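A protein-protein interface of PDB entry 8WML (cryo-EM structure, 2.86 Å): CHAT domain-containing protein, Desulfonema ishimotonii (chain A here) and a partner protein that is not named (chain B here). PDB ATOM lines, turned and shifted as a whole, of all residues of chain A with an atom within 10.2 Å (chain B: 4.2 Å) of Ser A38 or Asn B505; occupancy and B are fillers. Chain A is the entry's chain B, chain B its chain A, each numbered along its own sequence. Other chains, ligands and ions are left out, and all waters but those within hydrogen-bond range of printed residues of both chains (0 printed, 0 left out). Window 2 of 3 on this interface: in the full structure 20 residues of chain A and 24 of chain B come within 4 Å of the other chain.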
ATOM      1  N   TYR A  31      -5.666   7.263 -17.756  1.00  0.00           N
ATOM      2  CA  TYR A  31      -5.303   8.674 -17.846  1.00  0.00           C
ATOM      3  C   TYR A  31      -5.056   9.089 -19.291  1.00  0.00           C
ATOM      4  O   TYR A  31      -5.507  10.157 -19.727  1.00  0.00           O
ATOM      5  CB  TYR A  31      -4.068   8.956 -16.996  1.00  0.00           C
ATOM      6  CG  TYR A  31      -3.561  10.374 -17.113  1.00  0.00           C
ATOM      7  CD1 TYR A  31      -4.332  11.448 -16.690  1.00  0.00           C
ATOM      8  CD2 TYR A  31      -2.314  10.640 -17.662  1.00  0.00           C
ATOM      9  CE1 TYR A  31      -3.872  12.745 -16.803  1.00  0.00           C
ATOM     10  CE2 TYR A  31      -1.847  11.933 -17.779  1.00  0.00           C
ATOM     11  CZ  TYR A  31      -2.629  12.981 -17.349  1.00  0.00           C
ATOM     12  OH  TYR A  31      -2.163  14.269 -17.465  1.00  0.00           O
ATOM     13  N   GLU A  32      -4.346   8.251 -20.053  1.00  0.00           N
ATOM     14  CA  GLU A  32      -4.096   8.563 -21.457  1.00  0.00           C
ATOM     15  C   GLU A  32      -5.393   8.692 -22.238  1.00  0.00           C
ATOM     16  O   GLU A  32      -5.580   9.663 -22.978  1.00  0.00           O
ATOM     17  CB  GLU A  32      -3.214   7.488 -22.098  1.00  0.00           C
ATOM     18  CG  GLU A  32      -2.104   8.021 -23.011  1.00  0.00           C
ATOM     19  CD  GLU A  32      -2.514   8.144 -24.475  1.00  0.00           C
ATOM     20  OE1 GLU A  32      -3.641   7.746 -24.840  1.00  0.00           O
ATOM     21  OE2 GLU A  32      -1.694   8.644 -25.272  1.00  0.00           O
ATOM     22  N   LYS A  33      -6.304   7.731 -22.077  1.00  0.00           N
ATOM     23  CA  LYS A  33      -7.553   7.765 -22.830  1.00  0.00           C
ATOM     24  C   LYS A  33      -8.354   9.010 -22.479  1.00  0.00           C
ATOM     25  O   LYS A  33      -8.892   9.687 -23.364  1.00  0.00           O
ATOM     26  CB  LYS A  33      -8.364   6.501 -22.551  1.00  0.00           C
ATOM     27  CG  LYS A  33      -9.636   6.385 -23.375  1.00  0.00           C
ATOM     28  CD  LYS A  33     -10.317   5.047 -23.158  1.00  0.00           C
ATOM     29  CE  LYS A  33     -11.010   4.992 -21.810  1.00  0.00           C
ATOM     30  NZ  LYS A  33     -11.788   3.737 -21.663  1.00  0.00           N
ATOM     31  N   GLN A  34      -8.424   9.341 -21.186  1.00  0.00           N
ATOM     32  CA  GLN A  34      -9.123  10.555 -20.778  1.00  0.00           C
ATOM     33  C   GLN A  34      -8.463  11.799 -21.357  1.00  0.00           C
ATOM     34  O   GLN A  34      -9.142  12.801 -21.603  1.00  0.00           O
ATOM     35  CB  GLN A  34      -9.173  10.656 -19.253  1.00  0.00           C
ATOM     36  CG  GLN A  34      -9.924   9.529 -18.559  1.00  0.00           C
ATOM     37  CD  GLN A  34     -11.409   9.798 -18.459  1.00  0.00           C
ATOM     38  OE1 GLN A  34     -12.166   9.512 -19.386  1.00  0.00           O
ATOM     39  NE2 GLN A  34     -11.834  10.364 -17.336  1.00  0.00           N
ATOM     40  N   LEU A  35      -7.145  11.765 -21.566  1.00  0.00           N
ATOM     41  CA  LEU A  35      -6.490  12.899 -22.216  1.00  0.00           C
ATOM     42  C   LEU A  35      -6.877  12.992 -23.689  1.00  0.00           C
ATOM     43  O   LEU A  35      -7.121  14.091 -24.200  1.00  0.00           O
ATOM     44  CB  LEU A  35      -4.970  12.801 -22.070  1.00  0.00           C
ATOM     45  CG  LEU A  35      -4.308  13.614 -20.952  1.00  0.00           C
ATOM     46  CD1 LEU A  35      -2.825  13.292 -20.882  1.00  0.00           C
ATOM     47  CD2 LEU A  35      -4.509  15.114 -21.143  1.00  0.00           C
ATOM     48  N   MET A  36      -6.928  11.855 -24.391  1.00  0.00           N
ATOM     49  CA  MET A  36      -7.290  11.896 -25.810  1.00  0.00           C
ATOM     50  C   MET A  36      -8.726  12.371 -26.006  1.00  0.00           C
ATOM     51  O   MET A  36      -8.972  13.311 -26.771  1.00  0.00           O
ATOM     52  CB  MET A  36      -7.076  10.545 -26.511  1.00  0.00           C
ATOM     53  CG  MET A  36      -5.786   9.786 -26.218  1.00  0.00           C
ATOM     54  SD  MET A  36      -4.409  10.349 -27.237  1.00  0.00           S
ATOM     55  CE  MET A  36      -4.717   9.458 -28.760  1.00  0.00           C
ATOM     56  N   ASP A  37      -9.690  11.751 -25.324  1.00  0.00           N
ATOM     57  CA  ASP A  37     -11.087  12.155 -25.473  1.00  0.00           C
ATOM     58  C   ASP A  37     -11.373  13.295 -24.503  1.00  0.00           C
ATOM     59  O   ASP A  37     -11.120  13.175 -23.300  1.00  0.00           O
ATOM     60  CB  ASP A  37     -12.057  10.987 -25.262  1.00  0.00           C
ATOM     61  CG  ASP A  37     -12.002  10.397 -23.865  1.00  0.00           C
ATOM     62  OD1 ASP A  37     -12.567  11.005 -22.932  1.00  0.00           O
ATOM     63  OD2 ASP A  37     -11.444   9.293 -23.708  1.00  0.00           O
ATOM     64  N   SER A  38     -11.873  14.408 -25.029  1.00  0.00           N
ATOM     65  CA  SER A  38     -12.117  15.581 -24.203  1.00  0.00           C
ATOM     66  C   SER A  38     -13.239  15.308 -23.210  1.00  0.00           C
ATOM     67  O   SER A  38     -14.263  14.710 -23.551  1.00  0.00           O
ATOM     68  CB  SER A  38     -12.469  16.781 -25.080  1.00  0.00           C
ATOM     69  OG  SER A  38     -11.385  17.122 -25.926  1.00  0.00           O
ATOM     70  N   SER A  39     -13.042  15.751 -21.972  1.00  0.00           N
ATOM     71  CA  SER A  39     -14.004  15.507 -20.905  1.00  0.00           C
ATOM     72  C   SER A  39     -13.750  16.517 -19.794  1.00  0.00           C
ATOM     73  O   SER A  39     -12.850  17.355 -19.883  1.00  0.00           O
ATOM     74  CB  SER A  39     -13.899  14.067 -20.396  1.00  0.00           C
ATOM     75  OG  SER A  39     -12.602  13.799 -19.890  1.00  0.00           O
ATOM     76  N   GLU A  40     -14.563  16.431 -18.738  1.00  0.00           N
ATOM     77  CA  GLU A  40     -14.388  17.317 -17.592  1.00  0.00           C
ATOM     78  C   GLU A  40     -13.155  16.964 -16.769  1.00  0.00           C
ATOM     79  O   GLU A  40     -12.700  17.791 -15.975  1.00  0.00           O
ATOM     80  CB  GLU A  40     -15.627  17.287 -16.693  1.00  0.00           C
ATOM     81  CG  GLU A  40     -16.237  18.655 -16.438  1.00  0.00           C
ATOM     82  CD  GLU A  40     -17.394  18.608 -15.456  1.00  0.00           C
ATOM     83  OE1 GLU A  40     -17.402  19.415 -14.504  1.00  0.00           O
ATOM     84  OE2 GLU A  40     -18.296  17.764 -15.640  1.00  0.00           O
ATOM     85  N   ALA A  41     -12.604  15.760 -16.940  1.00  0.00           N
ATOM     86  CA  ALA A  41     -11.416  15.371 -16.192  1.00  0.00           C
ATOM     87  C   ALA A  41     -10.170  16.135 -16.624  1.00  0.00           C
ATOM     88  O   ALA A  41      -9.166  16.108 -15.908  1.00  0.00           O
ATOM     89  CB  ALA A  41     -11.173  13.869 -16.340  1.00  0.00           C
ATOM     90  N   THR A  42     -10.206  16.810 -17.776  1.00  0.00           N
ATOM     91  CA  THR A  42      -9.050  17.569 -18.237  1.00  0.00           C
ATOM     92  C   THR A  42      -8.851  18.876 -17.478  1.00  0.00           C
ATOM     93  O   THR A  42      -7.826  19.533 -17.681  1.00  0.00           O
ATOM     94  CB  THR A  42      -9.176  17.864 -19.733  1.00  0.00           C
ATOM     95  OG1 THR A  42     -10.503  18.317 -20.031  1.00  0.00           O
ATOM     96  CG2 THR A  42      -8.873  16.620 -20.547  1.00  0.00           C
ATOM     97  N   LEU A  43      -9.792  19.268 -16.619  1.00  0.00           N
ATOM     98  CA  LEU A  43      -9.644  20.469 -15.807  1.00  0.00           C
ATOM     99  C   LEU A  43      -8.786  20.251 -14.564  1.00  0.00           C
ATOM    100  O   LEU A  43      -8.562  21.208 -13.817  1.00  0.00           O
ATOM    101  CB  LEU A  43     -11.022  20.990 -15.391  1.00  0.00           C
ATOM    102  CG  LEU A  43     -11.816  21.738 -16.464  1.00  0.00           C
ATOM    103  CD1 LEU A  43     -13.289  21.787 -16.098  1.00  0.00           C
ATOM    104  CD2 LEU A  43     -11.273  23.145 -16.656  1.00  0.00           C
ATOM    105  N   CYS A  44      -8.311  19.031 -14.316  1.00  0.00           N
ATOM    106  CA  CYS A  44      -7.436  18.754 -13.181  1.00  0.00           C
ATOM    107  C   CYS A  44      -6.020  19.192 -13.537  1.00  0.00           C
ATOM    108  O   CYS A  44      -5.352  18.548 -14.353  1.00  0.00           O
ATOM    109  CB  CYS A  44      -7.481  17.271 -12.830  1.00  0.00           C
ATOM    110  SG  CYS A  44      -9.133  16.658 -12.436  1.00  0.00           S
ATOM    111  N   GLN A  45      -5.557  20.277 -12.914  1.00  0.00           N
ATOM    112  CA  GLN A  45      -4.318  20.951 -13.291  1.00  0.00           C
ATOM    113  C   GLN A  45      -3.205  20.749 -12.264  1.00  0.00           C
ATOM    114  O   GLN A  45      -2.359  21.629 -12.089  1.00  0.00           O
ATOM    115  CB  GLN A  45      -4.573  22.446 -13.491  1.00  0.00           C
ATOM    116  CG  GLN A  45      -5.620  22.798 -14.547  1.00  0.00           C
ATOM    117  CD  GLN A  45      -5.070  22.764 -15.959  1.00  0.00           C
ATOM    118  OE1 GLN A  45      -4.114  22.049 -16.247  1.00  0.00           O
ATOM    119  NE2 GLN A  45      -5.673  23.546 -16.846  1.00  0.00           N
ATOM    120  N   ARG B 503      -8.257  21.239 -33.345  1.00  0.00           N
ATOM    121  CA  ARG B 503      -9.477  21.042 -32.570  1.00  0.00           C
ATOM    122  C   ARG B 503      -9.262  21.613 -31.177  1.00  0.00           C
ATOM    123  O   ARG B 503      -8.237  21.342 -30.546  1.00  0.00           O
ATOM    124  CB  ARG B 503      -9.855  19.561 -32.484  1.00  0.00           C
ATOM    125  CG  ARG B 503     -11.246  19.311 -31.929  1.00  0.00           C
ATOM    126  CD  ARG B 503     -11.609  17.838 -31.965  1.00  0.00           C
ATOM    127  NE  ARG B 503     -10.948  17.092 -30.894  1.00  0.00           N
ATOM    128  CZ  ARG B 503     -10.107  16.070 -31.038  1.00  0.00           C
ATOM    129  NH1 ARG B 503      -9.758  15.602 -32.230  1.00  0.00           N
ATOM    130  NH2 ARG B 503      -9.596  15.498 -29.951  1.00  0.00           N
ATOM    131  N   ILE B 504     -10.230  22.396 -30.703  1.00  0.00           N
ATOM    132  CA  ILE B 504     -10.125  23.129 -29.445  1.00  0.00           C
ATOM    133  C   ILE B 504     -10.903  22.388 -28.368  1.00  0.00           C
ATOM    134  O   ILE B 504     -12.017  21.907 -28.607  1.00  0.00           O
ATOM    135  CB  ILE B 504     -10.642  24.574 -29.602  1.00  0.00           C
ATOM    136  CG1 ILE B 504      -9.759  25.377 -30.567  1.00  0.00           C
ATOM    137  CG2 ILE B 504     -10.721  25.271 -28.250  1.00  0.00           C
ATOM    138  CD1 ILE B 504      -8.419  25.814 -30.000  1.00  0.00           C
ATOM    139  N   ASN B 505     -10.311  22.291 -27.181  1.00  0.00           N
ATOM    140  CA  ASN B 505     -10.988  21.698 -26.034  1.00  0.00           C
ATOM    141  C   ASN B 505     -11.896  22.745 -25.393  1.00  0.00           C
ATOM    142  O   ASN B 505     -11.391  23.772 -24.926  1.00  0.00           O
ATOM    143  CB  ASN B 505      -9.964  21.199 -25.021  1.00  0.00           C
ATOM    144  CG  ASN B 505     -10.588  20.394 -23.899  1.00  0.00           C
ATOM    145  OD1 ASN B 505     -11.797  20.188 -23.866  1.00  0.00           O
ATOM    146  ND2 ASN B 505      -9.760  19.929 -22.974  1.00  0.00           N
ATOM    147  N   PRO B 506     -13.222  22.546 -25.348  1.00  0.00           N
ATOM    148  CA  PRO B 506     -14.087  23.616 -24.820  1.00  0.00           C
ATOM    149  C   PRO B 506     -13.928  23.873 -23.330  1.00  0.00           C
ATOM    150  O   PRO B 506     -14.348  24.938 -22.862  1.00  0.00           O
ATOM    151  CB  PRO B 506     -15.500  23.123 -25.152  1.00  0.00           C
ATOM    152  CG  PRO B 506     -15.380  21.662 -25.217  1.00  0.00           C
ATOM    153  CD  PRO B 506     -14.027  21.390 -25.790  1.00  0.00           C
ATOM    154  N   PHE B 507     -13.343  22.946 -22.570  1.00  0.00           N
ATOM    155  CA  PHE B 507     -13.223  23.130 -21.126  1.00  0.00           C
ATOM    156  C   PHE B 507     -12.064  24.058 -20.777  1.00  0.00           C
ATOM    157  O   PHE B 507     -12.263  25.115 -20.171  1.00  0.00           O
ATOM    158  CB  PHE B 507     -13.050  21.774 -20.439  1.00  0.00           C
ATOM    159  CG  PHE B 507     -14.268  20.897 -20.512  1.00  0.00           C
ATOM    160  CD1 PHE B 507     -15.382  21.170 -19.739  1.00  0.00           C
ATOM    161  CD2 PHE B 507     -14.295  19.799 -21.353  1.00  0.00           C
ATOM    162  CE1 PHE B 507     -16.499  20.365 -19.807  1.00  0.00           C
ATOM    163  CE2 PHE B 507     -15.411  18.993 -21.424  1.00  0.00           C
ATOM    164  CZ  PHE B 507     -16.514  19.276 -20.649  1.00  0.00           C
ATOM    165  N   THR B 508     -10.841  23.674 -21.150  1.00  0.00           N
ATOM    166  CA  THR B 508      -9.674  24.489 -20.828  1.00  0.00           C
ATOM    167  C   THR B 508      -9.547  25.706 -21.735  1.00  0.00           C
ATOM    168  O   THR B 508      -9.075  26.754 -21.286  1.00  0.00           O
ATOM    169  CB  THR B 508      -8.397  23.651 -20.921  1.00  0.00           C
ATOM    170  OG1 THR B 508      -8.185  23.239 -22.275  1.00  0.00           O
ATOM    171  CG2 THR B 508      -8.494  22.424 -20.029  1.00  0.00           C
ATOM    172  N   GLY B 509      -9.958  25.591 -22.995  1.00  0.00           N
ATOM    173  CA  GLY B 509      -9.815  26.659 -23.963  1.00  0.00           C
ATOM    174  C   GLY B 509      -8.581  26.582 -24.835  1.00  0.00           C
ATOM    175  O   GLY B 509      -8.262  27.567 -25.511  1.00  0.00           O
ATOM    176  N   THR B 510      -7.881  25.451 -24.843  1.00  0.00           N
ATOM    177  CA  THR B 510      -6.686  25.223 -25.646  1.00  0.00           C
ATOM    178  C   THR B 510      -6.911  24.007 -26.540  1.00  0.00           C
ATOM    179  O   THR B 510      -7.936  23.329 -26.455  1.00  0.00           O
ATOM    180  CB  THR B 510      -5.456  25.025 -24.753  1.00  0.00           C
ATOM    181  OG1 THR B 510      -5.686  23.937 -23.852  1.00  0.00           O
ATOM    182  CG2 THR B 510      -5.168  26.279 -23.953  1.00  0.00           C
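The side-chain amide oxygen (OD1) of Asn B505 sits close to the backbone NH (N) of Phe B507 (3.4 Å). N of Asn B505 is in hydrogen-bond range of O of Thr B510. OG1 of Thr B508 is in hydrogen-bond range of OG1 of Thr B510 (3.0 Å). The backbone carbonyl oxygen (O) of Ser A39 is in hydrogen-bond range of the side-chain hydroxyl (OG1) of Thr A42 (2.5 Å).
Of chain A, only Ser A38 (3.7 Å) and Thr A42 (3.4 Å) come within 4 Å of Asn B505. No residue of chain A comes within 4 Å of Pro B506. No residue of chain A comes within 4 Å of Gly B509. Of the printed residues of chain B, Ser A39 touches Phe B507. Printed residues of chain B within 4 Å of Glu A40: Phe B507 (3.8 Å). Of the printed residues of chain B, Thr A42 touches Asn B505 and Thr B508. Printed residues of chain A within 4 Å of Arg B503: Met A36. Gln A45 touches none of the printed residues of chain B. Ala A41 touches none of the printed residues of chain B. The nearest residue of chain A that does not touch Asn B505 is Ser A39 (5.0 Å). The nearest printed residue of chain A that does not touch Arg B503 is Ser A38 (4.7 Å).
Of the 8 printed residues of chain B, 4 touch a printed residue of chain A. Hydrophobic or aromatic side chains of chain B that line the printed part of chain A: Phe B507. Among the printed residues, 6 pairs touch across the chains.
The side-chain hydroxyl of Thr A42 is in hydrogen-bond range of the side-chain amide nitrogen of Asn B505 (3.4 Å).
Among the printed residues, merely in contact across the chains: Ser A39 with Phe B507 (3.2 Å), Ser A38 with Asn B505 (3.7 Å), Thr A42 with Thr B508 (3.8 Å), Glu A40 with Phe B507 (3.8 Å) and Met A36 with Arg B503 (3.9 Å).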
